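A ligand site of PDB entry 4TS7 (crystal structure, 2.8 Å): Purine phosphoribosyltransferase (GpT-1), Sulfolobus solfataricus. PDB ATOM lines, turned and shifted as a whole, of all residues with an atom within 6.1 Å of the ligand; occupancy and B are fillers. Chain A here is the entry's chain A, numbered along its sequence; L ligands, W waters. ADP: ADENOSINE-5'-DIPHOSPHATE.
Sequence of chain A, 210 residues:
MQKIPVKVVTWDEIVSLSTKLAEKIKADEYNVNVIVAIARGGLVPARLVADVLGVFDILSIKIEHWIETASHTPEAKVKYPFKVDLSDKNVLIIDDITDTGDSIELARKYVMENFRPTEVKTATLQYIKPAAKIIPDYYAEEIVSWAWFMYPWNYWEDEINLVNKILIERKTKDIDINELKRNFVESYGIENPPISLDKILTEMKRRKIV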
ATOM      1  N   ILE A  38      21.105  -9.964 -24.634  1.00  0.00           N
ATOM      2  CA  ILE A  38      21.945 -10.140 -25.788  1.00  0.00           C
ATOM      3  C   ILE A  38      21.046 -10.181 -27.013  1.00  0.00           C
ATOM      4  O   ILE A  38      20.187 -11.051 -27.120  1.00  0.00           O
ATOM      5  CB  ILE A  38      22.746 -11.421 -25.657  1.00  0.00           C
ATOM      6  CG1 ILE A  38      23.686 -11.307 -24.450  1.00  0.00           C
ATOM      7  CG2 ILE A  38      23.525 -11.689 -26.913  1.00  0.00           C
ATOM      8  CD1 ILE A  38      24.477 -12.574 -24.133  1.00  0.00           C
ATOM      9  N   GLY A  41      18.853 -12.860 -29.865  1.00  0.00           N
ATOM     10  CA  GLY A  41      18.313 -14.026 -29.197  1.00  0.00           C
ATOM     11  C   GLY A  41      17.684 -13.844 -27.825  1.00  0.00           C
ATOM     12  O   GLY A  41      16.730 -14.530 -27.471  1.00  0.00           O
ATOM     13  N   GLY A  42      18.214 -12.912 -27.038  1.00  0.00           N
ATOM     14  CA  GLY A  42      17.776 -12.752 -25.668  1.00  0.00           C
ATOM     15  C   GLY A  42      16.659 -11.747 -25.447  1.00  0.00           C
ATOM     16  O   GLY A  42      16.094 -11.695 -24.351  1.00  0.00           O
ATOM     17  N   HIS A  65      28.248 -12.946 -34.823  1.00  0.00           N
ATOM     18  CA  HIS A  65      28.990 -14.197 -34.786  1.00  0.00           C
ATOM     19  C   HIS A  65      29.716 -14.394 -36.095  1.00  0.00           C
ATOM     20  O   HIS A  65      29.099 -14.560 -37.144  1.00  0.00           O
ATOM     21  CB  HIS A  65      28.039 -15.347 -34.446  1.00  0.00           C
ATOM     22  CG  HIS A  65      27.282 -15.118 -33.164  1.00  0.00           C
ATOM     23  ND1 HIS A  65      26.081 -14.445 -33.114  1.00  0.00           N
ATOM     24  CD2 HIS A  65      27.598 -15.424 -31.884  1.00  0.00           C
ATOM     25  CE1 HIS A  65      25.678 -14.368 -31.867  1.00  0.00           C
ATOM     26  NE2 HIS A  65      26.581 -14.955 -31.091  1.00  0.00           N
ATOM     27  N   ALA A  76      33.069 -14.094 -31.602  1.00  0.00           N
ATOM     28  CA  ALA A  76      31.888 -13.324 -31.235  1.00  0.00           C
ATOM     29  C   ALA A  76      32.312 -11.869 -31.069  1.00  0.00           C
ATOM     30  O   ALA A  76      33.406 -11.588 -30.599  1.00  0.00           O
ATOM     31  CB  ALA A  76      31.311 -13.854 -29.967  1.00  0.00           C
ATOM     32  N   ASP A  95      20.261 -14.525 -22.454  1.00  0.00           N
ATOM     33  CA  ASP A  95      20.253 -14.983 -23.837  1.00  0.00           C
ATOM     34  C   ASP A  95      19.264 -16.133 -23.963  1.00  0.00           C
ATOM     35  O   ASP A  95      18.770 -16.630 -22.944  1.00  0.00           O
ATOM     36  CB  ASP A  95      21.654 -15.419 -24.286  1.00  0.00           C
ATOM     37  CG  ASP A  95      21.968 -15.045 -25.731  1.00  0.00           C
ATOM     38  OD1 ASP A  95      21.024 -14.683 -26.476  1.00  0.00           O
ATOM     39  OD2 ASP A  95      23.146 -15.097 -26.133  1.00  0.00           O
ATOM     40  N   ASP A  96      18.970 -16.551 -25.181  1.00  0.00           N
ATOM     41  CA  ASP A  96      18.058 -17.663 -25.412  1.00  0.00           C
ATOM     42  C   ASP A  96      18.614 -19.029 -24.962  1.00  0.00           C
ATOM     43  O   ASP A  96      17.978 -19.752 -24.194  1.00  0.00           O
ATOM     44  CB  ASP A  96      17.588 -17.701 -26.878  1.00  0.00           C
ATOM     45  CG  ASP A  96      18.730 -17.478 -27.886  1.00  0.00           C
ATOM     46  OD1 ASP A  96      19.923 -17.517 -27.495  1.00  0.00           O
ATOM     47  OD2 ASP A  96      18.403 -17.273 -29.073  1.00  0.00           O
ATOM     48  N   ILE A  97      19.819 -19.361 -25.417  1.00  0.00           N
ATOM     49  CA  ILE A  97      20.374 -20.685 -25.187  1.00  0.00           C
ATOM     50  C   ILE A  97      21.868 -20.596 -24.926  1.00  0.00           C
ATOM     51  O   ILE A  97      22.538 -19.755 -25.491  1.00  0.00           O
ATOM     52  CB  ILE A  97      20.093 -21.623 -26.399  1.00  0.00           C
ATOM     53  CG1 ILE A  97      20.582 -23.052 -26.143  1.00  0.00           C
ATOM     54  CG2 ILE A  97      20.698 -21.049 -27.683  1.00  0.00           C
ATOM     55  CD1 ILE A  97      19.989 -24.063 -27.095  1.00  0.00           C
ATOM     56  N   THR A  98      22.381 -21.459 -24.054  1.00  0.00           N
ATOM     57  CA  THR A  98      23.822 -21.611 -23.931  1.00  0.00           C
ATOM     58  C   THR A  98      24.204 -22.820 -24.766  1.00  0.00           C
ATOM     59  O   THR A  98      23.920 -23.959 -24.396  1.00  0.00           O
ATOM     60  CB  THR A  98      24.253 -21.821 -22.484  1.00  0.00           C
ATOM     61  OG1 THR A  98      23.897 -20.649 -21.730  1.00  0.00           O
ATOM     62  CG2 THR A  98      25.777 -22.040 -22.376  1.00  0.00           C
ATOM     63  N   ASP A  99      24.804 -22.567 -25.929  1.00  0.00           N
ATOM     64  CA  ASP A  99      25.253 -23.629 -26.818  1.00  0.00           C
ATOM     65  C   ASP A  99      26.760 -23.840 -26.658  1.00  0.00           C
ATOM     66  O   ASP A  99      27.197 -24.807 -26.035  1.00  0.00           O
ATOM     67  CB  ASP A  99      24.881 -23.304 -28.263  1.00  0.00           C
ATOM     68  CG  ASP A  99      25.152 -24.441 -29.209  1.00  0.00           C
ATOM     69  OD1 ASP A  99      24.467 -24.498 -30.252  1.00  0.00           O
ATOM     70  OD2 ASP A  99      26.037 -25.269 -28.927  1.00  0.00           O
ATOM     71  N   THR A 100      27.547 -22.901 -27.190  1.00  0.00           N
ATOM     72  CA  THR A 100      28.999 -22.989 -27.054  1.00  0.00           C
ATOM     73  C   THR A 100      29.431 -22.268 -25.805  1.00  0.00           C
ATOM     74  O   THR A 100      30.326 -22.716 -25.106  1.00  0.00           O
ATOM     75  CB  THR A 100      29.725 -22.380 -28.270  1.00  0.00           C
ATOM     76  OG1 THR A 100      29.529 -20.960 -28.281  1.00  0.00           O
ATOM     77  CG2 THR A 100      29.219 -22.974 -29.570  1.00  0.00           C
ATOM     78  N   GLY A 101      28.788 -21.131 -25.531  1.00  0.00           N
ATOM     79  CA  GLY A 101      29.134 -20.291 -24.388  1.00  0.00           C
ATOM     80  C   GLY A 101      29.937 -19.067 -24.794  1.00  0.00           C
ATOM     81  O   GLY A 101      30.259 -18.214 -23.968  1.00  0.00           O
ATOM     82  N   ASP A 102      30.236 -18.969 -26.088  1.00  0.00           N
ATOM     83  CA  ASP A 102      31.064 -17.893 -26.616  1.00  0.00           C
ATOM     84  C   ASP A 102      30.427 -16.511 -26.435  1.00  0.00           C
ATOM     85  O   ASP A 102      31.115 -15.520 -26.157  1.00  0.00           O
ATOM     86  CB  ASP A 102      31.407 -18.137 -28.085  1.00  0.00           C
ATOM     87  CG  ASP A 102      32.471 -19.216 -28.280  1.00  0.00           C
ATOM     88  OD1 ASP A 102      32.805 -19.941 -27.322  1.00  0.00           O
ATOM     89  OD2 ASP A 102      32.979 -19.343 -29.407  1.00  0.00           O
ATOM     90  N   SER A 103      29.106 -16.440 -26.596  1.00  0.00           N
ATOM     91  CA  SER A 103      28.417 -15.161 -26.517  1.00  0.00           C
ATOM     92  C   SER A 103      28.224 -14.682 -25.096  1.00  0.00           C
ATOM     93  O   SER A 103      28.412 -13.494 -24.812  1.00  0.00           O
ATOM     94  CB  SER A 103      27.069 -15.232 -27.222  1.00  0.00           C
ATOM     95  OG  SER A 103      27.220 -15.594 -28.576  1.00  0.00           O
ATOM     96  N   ILE A 104      27.858 -15.583 -24.201  1.00  0.00           N
ATOM     97  CA  ILE A 104      27.693 -15.170 -22.810  1.00  0.00           C
ATOM     98  C   ILE A 104      29.046 -14.925 -22.134  1.00  0.00           C
ATOM     99  O   ILE A 104      29.133 -14.182 -21.154  1.00  0.00           O
ATOM    100  CB  ILE A 104      26.833 -16.165 -21.981  1.00  0.00           C
ATOM    101  CG1 ILE A 104      27.411 -17.576 -22.066  1.00  0.00           C
ATOM    102  CG2 ILE A 104      25.421 -16.175 -22.497  1.00  0.00           C
ATOM    103  CD1 ILE A 104      26.801 -18.537 -21.059  1.00  0.00           C
ATOM    104  N   GLU A 105      30.099 -15.532 -22.661  1.00  0.00           N
ATOM    105  CA  GLU A 105      31.450 -15.244 -22.204  1.00  0.00           C
ATOM    106  C   GLU A 105      31.821 -13.807 -22.552  1.00  0.00           C
ATOM    107  O   GLU A 105      32.331 -13.064 -21.735  1.00  0.00           O
ATOM    108  CB  GLU A 105      32.458 -16.191 -22.820  1.00  0.00           C
ATOM    109  CG  GLU A 105      33.882 -15.954 -22.341  1.00  0.00           C
ATOM    110  CD  GLU A 105      34.900 -16.901 -22.979  1.00  0.00           C
ATOM    111  OE1 GLU A 105      34.907 -17.040 -24.221  1.00  0.00           O
ATOM    112  OE2 GLU A 105      35.706 -17.485 -22.230  1.00  0.00           O
ATOM    113  N   THR A 124      20.244 -18.250 -19.285  1.00  0.00           N
ATOM    114  CA  THR A 124      19.596 -18.585 -20.552  1.00  0.00           C
ATOM    115  C   THR A 124      18.446 -19.562 -20.323  1.00  0.00           C
ATOM    116  O   THR A 124      18.379 -20.244 -19.290  1.00  0.00           O
ATOM    117  CB  THR A 124      20.603 -19.187 -21.579  1.00  0.00           C
ATOM    118  OG1 THR A 124      21.171 -20.407 -21.066  1.00  0.00           O
ATOM    119  CG2 THR A 124      21.724 -18.200 -21.897  1.00  0.00           C
ATOM    120  N   ILE A 128      22.987 -26.506 -23.229  1.00  0.00           N
ATOM    121  CA  ILE A 128      23.371 -27.787 -23.822  1.00  0.00           C
ATOM    122  C   ILE A 128      24.650 -28.302 -23.190  1.00  0.00           C
ATOM    123  O   ILE A 128      25.741 -27.932 -23.606  1.00  0.00           O
ATOM    124  CB  ILE A 128      23.543 -27.699 -25.340  1.00  0.00           C
ATOM    125  CG1 ILE A 128      22.277 -27.124 -25.995  1.00  0.00           C
ATOM    126  CG2 ILE A 128      23.827 -29.076 -25.904  1.00  0.00           C
ATOM    127  CD1 ILE A 128      22.421 -26.819 -27.482  1.00  0.00           C
ATOM    128  N   TRP A 146      22.648 -32.306 -28.336  1.00  0.00           N
ATOM    129  CA  TRP A 146      22.538 -31.126 -29.192  1.00  0.00           C
ATOM    130  C   TRP A 146      21.471 -31.248 -30.246  1.00  0.00           C
ATOM    131  O   TRP A 146      21.370 -32.266 -30.927  1.00  0.00           O
ATOM    132  CB  TRP A 146      23.868 -30.829 -29.882  1.00  0.00           C
ATOM    133  CG  TRP A 146      23.893 -29.521 -30.635  1.00  0.00           C
ATOM    134  CD1 TRP A 146      24.443 -28.341 -30.218  1.00  0.00           C
ATOM    135  CD2 TRP A 146      23.349 -29.260 -31.938  1.00  0.00           C
ATOM    136  NE1 TRP A 146      24.283 -27.373 -31.176  1.00  0.00           N
ATOM    137  CE2 TRP A 146      23.613 -27.909 -32.243  1.00  0.00           C
ATOM    138  CE3 TRP A 146      22.677 -30.041 -32.884  1.00  0.00           C
ATOM    139  CZ2 TRP A 146      23.214 -27.316 -33.451  1.00  0.00           C
ATOM    140  CZ3 TRP A 146      22.282 -29.454 -34.086  1.00  0.00           C
ATOM    141  CH2 TRP A 146      22.554 -28.108 -34.355  1.00  0.00           C
ATOM    142  N   ALA A 147      20.697 -30.184 -30.394  1.00  0.00           N
ATOM    143  CA  ALA A 147      19.752 -30.021 -31.494  1.00  0.00           C
ATOM    144  C   ALA A 147      19.677 -28.541 -31.806  1.00  0.00           C
ATOM    145  O   ALA A 147      20.179 -27.716 -31.038  1.00  0.00           O
ATOM    146  CB  ALA A 147      18.382 -30.545 -31.106  1.00  0.00           C
ATOM    147  N   TRP A 148      19.076 -28.183 -32.941  1.00  0.00           N
ATOM    148  CA  TRP A 148      18.808 -26.779 -33.195  1.00  0.00           C
ATOM    149  C   TRP A 148      17.381 -26.468 -32.765  1.00  0.00           C
ATOM    150  O   TRP A 148      16.460 -27.144 -33.208  1.00  0.00           O
ATOM    151  CB  TRP A 148      19.016 -26.422 -34.659  1.00  0.00           C
ATOM    152  CG  TRP A 148      18.703 -24.982 -34.908  1.00  0.00           C
ATOM    153  CD1 TRP A 148      17.501 -24.451 -35.242  1.00  0.00           C
ATOM    154  CD2 TRP A 148      19.624 -23.879 -34.827  1.00  0.00           C
ATOM    155  NE1 TRP A 148      17.608 -23.088 -35.384  1.00  0.00           N
ATOM    156  CE2 TRP A 148      18.897 -22.717 -35.142  1.00  0.00           C
ATOM    157  CE3 TRP A 148      20.990 -23.762 -34.535  1.00  0.00           C
ATOM    158  CZ2 TRP A 148      19.482 -21.448 -35.146  1.00  0.00           C
ATOM    159  CZ3 TRP A 148      21.576 -22.511 -34.553  1.00  0.00           C
ATOM    160  CH2 TRP A 148      20.827 -21.368 -34.852  1.00  0.00           C
ATOM    161  N   PHE A 149      17.224 -25.470 -31.899  1.00  0.00           N
ATOM    162  CA  PHE A 149      15.901 -25.085 -31.372  1.00  0.00           C
ATOM    163  C   PHE A 149      15.270 -23.921 -32.120  1.00  0.00           C
ATOM    164  O   PHE A 149      15.775 -22.788 -32.097  1.00  0.00           O
ATOM    165  CB  PHE A 149      15.990 -24.788 -29.882  1.00  0.00           C
ATOM    166  CG  PHE A 149      16.377 -25.971 -29.077  1.00  0.00           C
ATOM    167  CD1 PHE A 149      17.709 -26.297 -28.875  1.00  0.00           C
ATOM    168  CD2 PHE A 149      15.407 -26.822 -28.559  1.00  0.00           C
ATOM    169  CE1 PHE A 149      18.072 -27.428 -28.147  1.00  0.00           C
ATOM    170  CE2 PHE A 149      15.761 -27.943 -27.830  1.00  0.00           C
ATOM    171  CZ  PHE A 149      17.091 -28.252 -27.627  1.00  0.00           C
ATOM    172  N   MET A 150      14.157 -24.185 -32.803  1.00  0.00           N
ATOM    173  CA  MET A 150      13.438 -23.145 -33.523  1.00  0.00           C
ATOM    174  C   MET A 150      12.548 -22.364 -32.562  1.00  0.00           C
ATOM    175  O   MET A 150      11.492 -22.863 -32.128  1.00  0.00           O
ATOM    176  CB  MET A 150      12.575 -23.723 -34.637  1.00  0.00           C
ATOM    177  CG  MET A 150      13.216 -23.673 -35.995  1.00  0.00           C
ATOM    178  SD  MET A 150      12.198 -24.409 -37.282  1.00  0.00           S
ATOM    179  CE  MET A 150      10.899 -23.193 -37.380  1.00  0.00           C
ATOM    180  N   TYR A 151      12.948 -21.156 -32.232  1.00  0.00           N
ATOM    181  CA  TYR A 151      12.140 -20.337 -31.335  1.00  0.00           C
ATOM    182  C   TYR A 151      11.049 -19.594 -32.110  1.00  0.00           C
ATOM    183  O   TYR A 151      11.237 -19.247 -33.267  1.00  0.00           O
ATOM    184  CB  TYR A 151      13.026 -19.389 -30.541  1.00  0.00           C
ATOM    185  CG  TYR A 151      14.072 -20.090 -29.713  1.00  0.00           C
ATOM    186  CD1 TYR A 151      15.424 -19.883 -29.937  1.00  0.00           C
ATOM    187  CD2 TYR A 151      13.710 -20.970 -28.697  1.00  0.00           C
ATOM    188  CE1 TYR A 151      16.394 -20.533 -29.173  1.00  0.00           C
ATOM    189  CE2 TYR A 151      14.661 -21.616 -27.946  1.00  0.00           C
ATOM    190  CZ  TYR A 151      16.003 -21.397 -28.184  1.00  0.00           C
ATOM    191  OH  TYR A 151      16.962 -22.037 -27.433  1.00  0.00           O
ATOM    192  N   ASN A 154      11.700 -16.716 -34.367  1.00  0.00           N
ATOM    193  CA  ASN A 154      12.817 -17.018 -35.254  1.00  0.00           C
ATOM    194  C   ASN A 154      12.368 -17.939 -36.396  1.00  0.00           C
ATOM    195  O   ASN A 154      13.167 -18.301 -37.263  1.00  0.00           O
ATOM    196  CB  ASN A 154      13.934 -17.695 -34.431  1.00  0.00           C
ATOM    197  CG  ASN A 154      15.324 -17.308 -34.886  1.00  0.00           C
ATOM    198  OD1 ASN A 154      16.183 -16.984 -34.062  1.00  0.00           O
ATOM    199  ND2 ASN A 154      15.570 -17.348 -36.204  1.00  0.00           N
ATOM    200  N   ASP A 158      14.763 -19.148 -39.531  1.00  0.00           N
ATOM    201  CA  ASP A 158      15.255 -20.500 -39.395  1.00  0.00           C
ATOM    202  C   ASP A 158      14.806 -21.362 -40.565  1.00  0.00           C
ATOM    203  O   ASP A 158      15.596 -22.128 -41.121  1.00  0.00           O
ATOM    204  CB  ASP A 158      14.777 -21.126 -38.087  1.00  0.00           C
ATOM    205  CG  ASP A 158      15.665 -20.755 -36.904  1.00  0.00           C
ATOM    206  OD1 ASP A 158      16.819 -20.364 -37.126  1.00  0.00           O
ATOM    207  OD2 ASP A 158      15.192 -20.881 -35.751  1.00  0.00           O
HETATM  208  PB  ADP L   1      25.904 -18.834 -26.122  1.00  0.00           P
HETATM  209  O1B ADP L   1      24.621 -18.365 -25.498  1.00  0.00           O
HETATM  210  O2B ADP L   1      26.163 -20.318 -26.017  1.00  0.00           O
HETATM  211  O3B ADP L   1      27.064 -17.925 -25.798  1.00  0.00           O
HETATM  212  PA  ADP L   1      26.447 -19.192 -28.948  1.00  0.00           P
HETATM  213  O1A ADP L   1      27.573 -18.245 -29.302  1.00  0.00           O
HETATM  214  O2A ADP L   1      26.714 -20.664 -28.780  1.00  0.00           O
HETATM  215  O3A ADP L   1      25.643 -18.573 -27.690  1.00  0.00           O
HETATM  216  O5' ADP L   1      25.292 -19.015 -30.024  1.00  0.00           O
HETATM  217  C5' ADP L   1      24.972 -17.685 -30.401  1.00  0.00           C
HETATM  218  C4' ADP L   1      23.518 -17.577 -30.834  1.00  0.00           C
HETATM  219  O4' ADP L   1      23.240 -18.517 -31.870  1.00  0.00           O
HETATM  220  C3' ADP L   1      22.503 -17.847 -29.737  1.00  0.00           C
HETATM  221  O3' ADP L   1      22.144 -16.635 -29.067  1.00  0.00           O
HETATM  222  C2' ADP L   1      21.313 -18.425 -30.477  1.00  0.00           C
HETATM  223  O2' ADP L   1      20.437 -17.380 -30.936  1.00  0.00           O
HETATM  224  C1' ADP L   1      21.941 -19.067 -31.706  1.00  0.00           C
HETATM  225  N9  ADP L   1      22.082 -20.523 -31.457  1.00  0.00           N
HETATM  226  C8  ADP L   1      23.238 -21.197 -31.248  1.00  0.00           C
HETATM  227  N7  ADP L   1      23.004 -22.532 -31.059  1.00  0.00           N
HETATM  228  C5  ADP L   1      21.673 -22.717 -31.149  1.00  0.00           C
HETATM  229  C6  ADP L   1      20.746 -23.857 -31.059  1.00  0.00           C
HETATM  230  N6  ADP L   1      21.195 -25.103 -30.821  1.00  0.00           N
HETATM  231  N1  ADP L   1      19.427 -23.617 -31.206  1.00  0.00           N
HETATM  232  C2  ADP L   1      18.949 -22.367 -31.435  1.00  0.00           C
HETATM  233  N3  ADP L   1      19.732 -21.276 -31.541  1.00  0.00           N
HETATM  234  C4  ADP L   1      21.070 -21.386 -31.410  1.00  0.00           C
HETATM  235  O   HOH W   1      24.383 -14.862 -28.781  1.00  0.00           O
HETATM  236  O   HOH W   2      23.155 -17.453 -35.118  1.00  0.00           O
HETATM  237  O   HOH W   3      18.088 -19.213 -32.745  1.00  0.00           O
HETATM  238  O   HOH W   4      26.645 -21.670 -31.862  1.00  0.00           O
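OD1 of Asp 95 lies within hydrogen-bond range of N of Gly 42 (3.4 Å).
The side-chain hydroxyl (OG1) of Thr 124 lies within hydrogen-bond range of the side-chain hydroxyl (OG1) of Thr 98, 2.8 Å away.
OD1 of Asp 99 lies within hydrogen-bond range of NE1 of Trp 146, 3.0 Å away.
The side-chain hydroxyl (OG) of Ser 103 sits at hydrogen-bond distance from a ring nitrogen (NE2) of His 65 (2.7 Å).
The indole nitrogen (NE1) of Trp 148 sits at hydrogen-bond distance from the side-chain carboxylate (OD2) of Asp 158, at 3.3 Å.
N of Ile 128 is in hydrogen-bond range of O of Thr 98, at 3.0 Å.
The side-chain hydroxyl (OG1) of Thr 100 is in hydrogen-bond range of the backbone NH (N) of Asp 102 (3.0 Å).
Merely in contact with the ligand: His 65 (3.2 Å), Trp 148 (3.4 Å), Thr 98 (3.4 Å), Trp 146 (3.8 Å), Tyr 151 (3.9 Å) and Ile 128 (3.9 Å).
Hydrophobic or aromatic side chains within 4 Å of the ligand: His 65, Ile 97, Ile 104, Ile 128, Trp 146, Trp 148, Phe 149 and Tyr 151.
The nearest printed residue that does not touch the ligand is Gly 41 (4.3 Å).
Water W1 lies within hydrogen-bond range of an oxygen (O3') of the ligand, the side-chain carboxylate of Asp 95, the side-chain hydroxyl of Ser 103 and a ring nitrogen (NE2) of His 65.
Water W3 lies within hydrogen-bond range of N3 of the ligand (2.9 Å) and OD1 of Asn 154 (3.2 Å).
The backbone NH (N) of Gly 101 sits at hydrogen-bond distance from an oxygen (O2B) of the ligand, 2.8 Å away.
OG1 of Thr 100 sits at hydrogen-bond distance from O2A of the ligand.
OG of Ser 103 is in hydrogen-bond range of O1A of the ligand (2.8 Å).
The backbone NH (N) of Ile 104 lies within hydrogen-bond range of an oxygen (O3B) of the ligand.
N7 of the ligand sits at hydrogen-bond distance from OD1 of Asp 99, 2.6 Å away.
The backbone NH (N) of Phe 149 is in hydrogen-bond range of a nitrogen (N1) of the ligand, at 3.0 Å.
The backbone NH (N) of Asp 102 is in hydrogen-bond range of an oxygen (O3B) of the ligand (3.4 Å).
OD1 of Asp 95 is in hydrogen-bond range of O3' of the ligand (3.4 Å).
O of Ala 147 lies within hydrogen-bond range of N6 of the ligand, at 2.8 Å.
OD2 of Asp 96 lies within hydrogen-bond range of O2' of the ligand (2.8 Å).
The backbone NH of Thr 100 lies within hydrogen-bond range of an oxygen (O2A) of the ligand, at 2.9 Å.
O3B of the ligand lies within hydrogen-bond range of N of Ser 103 (2.6 Å).
O1B of the ligand lies close to O of Ile 97, 2.5 Å away.
The backbone NH (N) of Asp 99 is in hydrogen-bond range of an oxygen (O2B) of the ligand, at 2.6 Å.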
